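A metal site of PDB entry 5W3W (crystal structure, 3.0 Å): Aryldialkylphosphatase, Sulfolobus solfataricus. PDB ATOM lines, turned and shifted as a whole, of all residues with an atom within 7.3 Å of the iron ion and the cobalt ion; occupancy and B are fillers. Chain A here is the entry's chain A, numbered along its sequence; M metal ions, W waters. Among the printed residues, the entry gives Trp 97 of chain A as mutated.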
ATOM      1  N   HIS A  22     -15.614  15.578 -15.667  1.00  0.00           N
ATOM      2  CA  HIS A  22     -16.112  14.407 -14.965  1.00  0.00           C
ATOM      3  C   HIS A  22     -17.240  13.781 -15.812  1.00  0.00           C
ATOM      4  O   HIS A  22     -18.409  14.171 -15.752  1.00  0.00           O
ATOM      5  CB  HIS A  22     -16.563  14.835 -13.548  1.00  0.00           C
ATOM      6  CG  HIS A  22     -16.703  13.686 -12.596  1.00  0.00           C
ATOM      7  ND1 HIS A  22     -16.057  13.647 -11.377  1.00  0.00           N
ATOM      8  CD2 HIS A  22     -17.412  12.539 -12.684  1.00  0.00           C
ATOM      9  CE1 HIS A  22     -16.342  12.514 -10.764  1.00  0.00           C
ATOM     10  NE2 HIS A  22     -17.251  11.863 -11.478  1.00  0.00           N
ATOM     11  N   GLU A  23     -16.888  12.811 -16.629  1.00  0.00           N
ATOM     12  CA  GLU A  23     -17.888  11.991 -17.340  1.00  0.00           C
ATOM     13  C   GLU A  23     -17.443  10.504 -17.402  1.00  0.00           C
ATOM     14  O   GLU A  23     -16.255  10.176 -17.535  1.00  0.00           O
ATOM     15  CB  GLU A  23     -18.117  12.507 -18.742  1.00  0.00           C
ATOM     16  CG  GLU A  23     -18.468  13.968 -18.855  1.00  0.00           C
ATOM     17  CD  GLU A  23     -19.840  14.267 -18.333  1.00  0.00           C
ATOM     18  OE1 GLU A  23     -20.129  15.464 -18.120  1.00  0.00           O
ATOM     19  OE2 GLU A  23     -20.612  13.305 -18.138  1.00  0.00           O
ATOM     20  N   HIS A  24     -18.400   9.596 -17.294  1.00  0.00           N
ATOM     21  CA  HIS A  24     -18.084   8.135 -17.261  1.00  0.00           C
ATOM     22  C   HIS A  24     -18.639   7.488 -18.527  1.00  0.00           C
ATOM     23  O   HIS A  24     -19.866   7.426 -18.745  1.00  0.00           O
ATOM     24  CB  HIS A  24     -18.700   7.427 -16.032  1.00  0.00           C
ATOM     25  CG  HIS A  24     -18.237   7.968 -14.699  1.00  0.00           C
ATOM     26  ND1 HIS A  24     -17.112   7.483 -14.055  1.00  0.00           N
ATOM     27  CD2 HIS A  24     -18.768   8.924 -13.889  1.00  0.00           C
ATOM     28  CE1 HIS A  24     -16.941   8.157 -12.917  1.00  0.00           C
ATOM     29  NE2 HIS A  24     -18.008   8.941 -12.737  1.00  0.00           N
ATOM     30  N   PRO A  67     -13.121   9.641 -14.845  1.00  0.00           N
ATOM     31  CA  PRO A  67     -12.525   9.232 -13.571  1.00  0.00           C
ATOM     32  C   PRO A  67     -12.975   7.830 -13.097  1.00  0.00           C
ATOM     33  O   PRO A  67     -12.994   7.530 -11.879  1.00  0.00           O
ATOM     34  CB  PRO A  67     -12.943  10.367 -12.619  1.00  0.00           C
ATOM     35  CG  PRO A  67     -14.209  10.876 -13.174  1.00  0.00           C
ATOM     36  CD  PRO A  67     -14.281  10.511 -14.658  1.00  0.00           C
ATOM     37  N   THR A  68     -13.254   6.948 -14.057  1.00  0.00           N
ATOM     38  CA  THR A  68     -13.611   5.582 -13.790  1.00  0.00           C
ATOM     39  C   THR A  68     -12.334   4.843 -13.385  1.00  0.00           C
ATOM     40  O   THR A  68     -11.418   4.721 -14.191  1.00  0.00           O
ATOM     41  CB  THR A  68     -14.196   4.922 -15.053  1.00  0.00           C
ATOM     42  OG1 THR A  68     -15.347   5.654 -15.494  1.00  0.00           O
ATOM     43  CG2 THR A  68     -14.651   3.551 -14.733  1.00  0.00           C
ATOM     44  N   LEU A  72     -15.193   0.945 -10.048  1.00  0.00           N
ATOM     45  CA  LEU A  72     -16.103   1.441 -11.049  1.00  0.00           C
ATOM     46  C   LEU A  72     -15.908   0.762 -12.395  1.00  0.00           C
ATOM     47  O   LEU A  72     -16.579   1.092 -13.372  1.00  0.00           O
ATOM     48  CB  LEU A  72     -15.920   2.967 -11.191  1.00  0.00           C
ATOM     49  CG  LEU A  72     -16.263   3.841  -9.941  1.00  0.00           C
ATOM     50  CD1 LEU A  72     -15.875   5.302 -10.064  1.00  0.00           C
ATOM     51  CD2 LEU A  72     -17.754   3.769  -9.655  1.00  0.00           C
ATOM     52  N   TRP A  97     -11.829   3.640  -5.791  1.00  0.00           N
ATOM     53  CA  TRP A  97     -13.148   4.105  -5.426  1.00  0.00           C
ATOM     54  C   TRP A  97     -13.766   3.240  -4.315  1.00  0.00           C
ATOM     55  O   TRP A  97     -14.355   2.162  -4.587  1.00  0.00           O
ATOM     56  CB  TRP A  97     -14.024   4.072  -6.682  1.00  0.00           C
ATOM     57  CG  TRP A  97     -15.211   4.962  -6.583  1.00  0.00           C
ATOM     58  CD1 TRP A  97     -15.249   6.249  -6.879  1.00  0.00           C
ATOM     59  CD2 TRP A  97     -16.524   4.603  -6.142  1.00  0.00           C
ATOM     60  NE1 TRP A  97     -16.489   6.757  -6.665  1.00  0.00           N
ATOM     61  CE2 TRP A  97     -17.305   5.774  -6.205  1.00  0.00           C
ATOM     62  CE3 TRP A  97     -17.123   3.415  -5.704  1.00  0.00           C
ATOM     63  CZ2 TRP A  97     -18.660   5.817  -5.881  1.00  0.00           C
ATOM     64  CZ3 TRP A  97     -18.485   3.429  -5.367  1.00  0.00           C
ATOM     65  CH2 TRP A  97     -19.234   4.635  -5.463  1.00  0.00           C
ATOM     66  N   TYR A  99     -15.899   3.480  -0.168  1.00  0.00           N
ATOM     67  CA  TYR A  99     -16.556   4.254   0.903  1.00  0.00           C
ATOM     68  C   TYR A  99     -16.132   3.857   2.301  1.00  0.00           C
ATOM     69  O   TYR A  99     -15.985   4.712   3.167  1.00  0.00           O
ATOM     70  CB  TYR A  99     -18.078   4.169   0.814  1.00  0.00           C
ATOM     71  CG  TYR A  99     -18.675   4.793  -0.418  1.00  0.00           C
ATOM     72  CD1 TYR A  99     -17.955   5.744  -1.192  1.00  0.00           C
ATOM     73  CD2 TYR A  99     -19.976   4.511  -0.787  1.00  0.00           C
ATOM     74  CE1 TYR A  99     -18.517   6.336  -2.312  1.00  0.00           C
ATOM     75  CE2 TYR A  99     -20.547   5.104  -1.904  1.00  0.00           C
ATOM     76  CZ  TYR A  99     -19.829   6.020  -2.653  1.00  0.00           C
ATOM     77  OH  TYR A  99     -20.424   6.596  -3.747  1.00  0.00           O
ATOM     78  N   KCX A 137      -7.827   9.279  -8.884  1.00  0.00           N
ATOM     79  CA  KCX A 137      -9.154   9.438  -8.290  1.00  0.00           C
ATOM     80  CB  KCX A 137     -10.218   8.743  -9.173  1.00  0.00           C
ATOM     81  CG  KCX A 137     -11.526   9.564  -9.234  1.00  0.00           C
ATOM     82  CD  KCX A 137     -12.468   9.178  -8.129  1.00  0.00           C
ATOM     83  CE  KCX A 137     -13.738   9.977  -8.237  1.00  0.00           C
ATOM     84  NZ  KCX A 137     -14.654   9.428  -9.276  1.00  0.00           N
ATOM     85  C   KCX A 137      -9.307   8.869  -6.908  1.00  0.00           C
ATOM     86  O   KCX A 137      -8.968   7.733  -6.682  1.00  0.00           O
ATOM     87  CX  KCX A 137     -15.969   9.680  -9.287  1.00  0.00           C
ATOM     88  OQ1 KCX A 137     -16.487  10.394  -8.446  1.00  0.00           O
ATOM     89  OQ2 KCX A 137     -16.650   9.157 -10.240  1.00  0.00           O
ATOM     90  N   ILE A 138      -9.870   9.640  -5.975  1.00  0.00           N
ATOM     91  CA  ILE A 138     -10.188   9.117  -4.651  1.00  0.00           C
ATOM     92  C   ILE A 138     -11.639   9.440  -4.281  1.00  0.00           C
ATOM     93  O   ILE A 138     -12.259  10.272  -4.930  1.00  0.00           O
ATOM     94  CB  ILE A 138      -9.183   9.587  -3.564  1.00  0.00           C
ATOM     95  CG1 ILE A 138      -9.245  11.090  -3.312  1.00  0.00           C
ATOM     96  CG2 ILE A 138      -7.788   9.176  -3.984  1.00  0.00           C
ATOM     97  CD1 ILE A 138     -10.335  11.502  -2.341  1.00  0.00           C
ATOM     98  N   ALA A 139     -12.159   8.793  -3.249  1.00  0.00           N
ATOM     99  CA  ALA A 139     -13.564   8.975  -2.873  1.00  0.00           C
ATOM    100  C   ALA A 139     -13.755   8.962  -1.346  1.00  0.00           C
ATOM    101  O   ALA A 139     -12.815   8.687  -0.581  1.00  0.00           O
ATOM    102  CB  ALA A 139     -14.468   7.921  -3.559  1.00  0.00           C
ATOM    103  N   ASP A 141     -17.728   9.247   1.305  1.00  0.00           N
ATOM    104  CA  ASP A 141     -19.169   9.471   1.254  1.00  0.00           C
ATOM    105  C   ASP A 141     -19.738   9.352   2.668  1.00  0.00           C
ATOM    106  O   ASP A 141     -19.006   9.611   3.605  1.00  0.00           O
ATOM    107  CB  ASP A 141     -19.784   8.493   0.253  1.00  0.00           C
ATOM    108  CG  ASP A 141     -21.069   9.001  -0.329  1.00  0.00           C
ATOM    109  OD1 ASP A 141     -22.013   9.220   0.493  1.00  0.00           O
ATOM    110  OD2 ASP A 141     -21.149   9.175  -1.570  1.00  0.00           O
ATOM    111  N   THR A 169     -11.636  14.102  -6.859  1.00  0.00           N
ATOM    112  CA  THR A 169     -12.218  13.377  -5.723  1.00  0.00           C
ATOM    113  C   THR A 169     -13.697  13.208  -5.882  1.00  0.00           C
ATOM    114  O   THR A 169     -14.318  13.904  -6.679  1.00  0.00           O
ATOM    115  CB  THR A 169     -11.929  14.064  -4.370  1.00  0.00           C
ATOM    116  OG1 THR A 169     -12.844  15.142  -4.191  1.00  0.00           O
ATOM    117  CG2 THR A 169     -10.460  14.544  -4.293  1.00  0.00           C
ATOM    118  N   HIS A 170     -14.240  12.268  -5.109  1.00  0.00           N
ATOM    119  CA  HIS A 170     -15.687  12.060  -4.929  1.00  0.00           C
ATOM    120  C   HIS A 170     -16.009  12.283  -3.441  1.00  0.00           C
ATOM    121  O   HIS A 170     -15.418  11.652  -2.537  1.00  0.00           O
ATOM    122  CB  HIS A 170     -16.042  10.673  -5.410  1.00  0.00           C
ATOM    123  CG  HIS A 170     -17.391  10.164  -4.991  1.00  0.00           C
ATOM    124  ND1 HIS A 170     -18.401   9.931  -5.910  1.00  0.00           N
ATOM    125  CD2 HIS A 170     -17.910   9.881  -3.763  1.00  0.00           C
ATOM    126  CE1 HIS A 170     -19.427   9.402  -5.258  1.00  0.00           C
ATOM    127  NE2 HIS A 170     -19.174   9.398  -3.956  1.00  0.00           N
ATOM    128  N   SER A 171     -16.922  13.192  -3.165  1.00  0.00           N
ATOM    129  CA  SER A 171     -17.230  13.546  -1.796  1.00  0.00           C
ATOM    130  C   SER A 171     -18.730  13.656  -1.631  1.00  0.00           C
ATOM    131  O   SER A 171     -19.475  13.653  -2.594  1.00  0.00           O
ATOM    132  CB  SER A 171     -16.495  14.852  -1.376  1.00  0.00           C
ATOM    133  OG  SER A 171     -16.913  15.989  -2.134  1.00  0.00           O
ATOM    134  N   GLY A 198     -14.955  17.141  -5.753  1.00  0.00           N
ATOM    135  CA  GLY A 198     -16.131  16.934  -6.599  1.00  0.00           C
ATOM    136  C   GLY A 198     -17.398  16.649  -5.833  1.00  0.00           C
ATOM    137  O   GLY A 198     -17.411  16.399  -4.625  1.00  0.00           O
ATOM    138  N   HIS A 199     -18.469  16.772  -6.591  1.00  0.00           N
ATOM    139  CA  HIS A 199     -19.844  16.548  -6.138  1.00  0.00           C
ATOM    140  C   HIS A 199     -20.377  17.561  -5.161  1.00  0.00           C
ATOM    141  O   HIS A 199     -21.460  17.374  -4.576  1.00  0.00           O
ATOM    142  CB  HIS A 199     -20.038  15.117  -5.618  1.00  0.00           C
ATOM    143  CG  HIS A 199     -19.524  14.073  -6.556  1.00  0.00           C
ATOM    144  ND1 HIS A 199     -19.756  14.099  -7.928  1.00  0.00           N
ATOM    145  CD2 HIS A 199     -18.775  12.968  -6.320  1.00  0.00           C
ATOM    146  CE1 HIS A 199     -19.176  13.045  -8.482  1.00  0.00           C
ATOM    147  NE2 HIS A 199     -18.640  12.309  -7.522  1.00  0.00           N
ATOM    148  N   ASP A 222     -20.379  19.138 -10.616  1.00  0.00           N
ATOM    149  CA  ASP A 222     -20.128  18.120 -11.662  1.00  0.00           C
ATOM    150  C   ASP A 222     -21.220  17.081 -11.830  1.00  0.00           C
ATOM    151  O   ASP A 222     -21.013  16.142 -12.538  1.00  0.00           O
ATOM    152  CB  ASP A 222     -18.808  17.396 -11.352  1.00  0.00           C
ATOM    153  CG  ASP A 222     -18.762  16.962  -9.926  1.00  0.00           C
ATOM    154  OD1 ASP A 222     -19.867  16.869  -9.371  1.00  0.00           O
ATOM    155  OD2 ASP A 222     -17.685  16.798  -9.322  1.00  0.00           O
ATOM    156  N   ARG A 223     -22.386  17.253 -11.223  1.00  0.00           N
ATOM    157  CA  ARG A 223     -23.500  16.295 -11.394  1.00  0.00           C
ATOM    158  C   ARG A 223     -24.788  16.930 -11.979  1.00  0.00           C
ATOM    159  O   ARG A 223     -25.931  16.715 -11.488  1.00  0.00           O
ATOM    160  CB  ARG A 223     -23.800  15.675 -10.049  1.00  0.00           C
ATOM    161  CG  ARG A 223     -22.816  14.597  -9.661  1.00  0.00           C
ATOM    162  CD  ARG A 223     -23.192  14.052  -8.288  1.00  0.00           C
ATOM    163  NE  ARG A 223     -22.509  12.784  -8.038  1.00  0.00           N
ATOM    164  CZ  ARG A 223     -22.456  12.155  -6.873  1.00  0.00           C
ATOM    165  NH1 ARG A 223     -23.062  12.643  -5.787  1.00  0.00           N
ATOM    166  NH2 ARG A 223     -21.766  11.020  -6.797  1.00  0.00           N
ATOM    167  N   HIS A 255     -21.298  16.594 -15.731  1.00  0.00           N
ATOM    168  CA  HIS A 255     -22.533  15.874 -15.566  1.00  0.00           C
ATOM    169  C   HIS A 255     -22.398  14.673 -14.643  1.00  0.00           C
ATOM    170  O   HIS A 255     -23.385  14.365 -13.920  1.00  0.00           O
ATOM    171  CB  HIS A 255     -23.044  15.394 -16.919  1.00  0.00           C
ATOM    172  CG  HIS A 255     -23.201  16.492 -17.918  1.00  0.00           C
ATOM    173  ND1 HIS A 255     -22.156  16.931 -18.685  1.00  0.00           N
ATOM    174  CD2 HIS A 255     -24.265  17.263 -18.244  1.00  0.00           C
ATOM    175  CE1 HIS A 255     -22.583  17.906 -19.480  1.00  0.00           C
ATOM    176  NE2 HIS A 255     -23.859  18.113 -19.230  1.00  0.00           N
ATOM    177  N   ASP A 256     -21.233  14.009 -14.665  1.00  0.00           N
ATOM    178  CA  ASP A 256     -21.002  12.708 -13.945  1.00  0.00           C
ATOM    179  C   ASP A 256     -21.888  11.634 -14.539  1.00  0.00           C
ATOM    180  O   ASP A 256     -22.284  10.698 -13.868  1.00  0.00           O
ATOM    181  CB  ASP A 256     -21.215  12.831 -12.417  1.00  0.00           C
ATOM    182  CG  ASP A 256     -20.645  11.644 -11.609  1.00  0.00           C
ATOM    183  OD1 ASP A 256     -19.837  10.877 -12.118  1.00  0.00           O
ATOM    184  OD2 ASP A 256     -21.001  11.462 -10.423  1.00  0.00           O
ATOM    185  N   TYR A 257     -22.177  11.780 -15.818  1.00  0.00           N
ATOM    186  CA  TYR A 257     -23.072  10.886 -16.533  1.00  0.00           C
ATOM    187  C   TYR A 257     -22.421   9.514 -16.767  1.00  0.00           C
ATOM    188  O   TYR A 257     -21.216   9.419 -16.971  1.00  0.00           O
ATOM    189  CB  TYR A 257     -23.485  11.517 -17.845  1.00  0.00           C
ATOM    190  CG  TYR A 257     -24.508  10.733 -18.631  1.00  0.00           C
ATOM    191  CD1 TYR A 257     -25.834  10.639 -18.186  1.00  0.00           C
ATOM    192  CD2 TYR A 257     -24.178  10.116 -19.840  1.00  0.00           C
ATOM    193  CE1 TYR A 257     -26.789   9.924 -18.917  1.00  0.00           C
ATOM    194  CE2 TYR A 257     -25.123   9.401 -20.575  1.00  0.00           C
ATOM    195  CZ  TYR A 257     -26.435   9.315 -20.115  1.00  0.00           C
ATOM    196  OH  TYR A 257     -27.383   8.619 -20.823  1.00  0.00           O
ATOM    197  N   CYS A 258     -23.269   8.481 -16.722  1.00  0.00           N
ATOM    198  CA  CYS A 258     -22.876   7.081 -16.912  1.00  0.00           C
ATOM    199  C   CYS A 258     -23.692   6.472 -18.036  1.00  0.00           C
ATOM    200  O   CYS A 258     -24.829   6.018 -17.812  1.00  0.00           O
ATOM    201  CB  CYS A 258     -23.144   6.258 -15.645  1.00  0.00           C
ATOM    202  SG  CYS A 258     -22.574   6.973 -14.088  1.00  0.00           S
HETATM  203 FE    FE M   1     -18.244  10.068 -11.059  1.00  0.00          FE
HETATM  204 CO    CO M   2     -18.299  10.411  -7.908  1.00  0.00          CO
HETATM  205  O   HOH W   1     -19.675   9.106  -9.601  1.00  0.00           O
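Of the 23 residues printed, 4 come within 4 Å of the iron ion.
The iron ion is bound by OQ2 of KCX 137, a ring nitrogen (NE2) of His 24, the side-chain carboxylate of Asp 256, a ring nitrogen (NE2) of His 22 and water W1.
OQ1 of KCX 137 binds the cobalt ion (1.9 Å). NE2 of His 199 is bound to the cobalt ion, 2.0 Å away. ND1 of His 170 binds the cobalt ion (2.1 Å). Water W1 binds the cobalt ion (2.5 Å).
Arg 223 touches the cobalt ion. Six residues have an atom within 4 Å of the cobalt ion: His 22, KCX 137, His 170, His 199, Arg 223 and Asp 256.
ND1 of His 199 is in hydrogen-bond range of NE of Arg 223, 3.1 Å away. The backbone NH of His 24 is in hydrogen-bond range of the backbone carbonyl oxygen of Tyr 257, 2.8 Å away. OG1 of Thr 68 lies within hydrogen-bond range of ND1 of His 24 (2.9 Å). NE2 of His 170 lies within hydrogen-bond range of OH of Tyr 99, at 3.1 Å. The backbone carbonyl oxygen (O) of Ile 138 lies within hydrogen-bond range of the backbone NH (N) of His 170 (2.8 Å). A ring nitrogen (NE2) of His 170 is in hydrogen-bond range of the side-chain carboxylate of Asp 141 (3.1 Å). OD2 of Asp 256 lies within salt-bridge range of NE of Arg 223 (3.1 Å). N of Asp 256 sits at hydrogen-bond distance from O of Asp 222 (3.0 Å).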
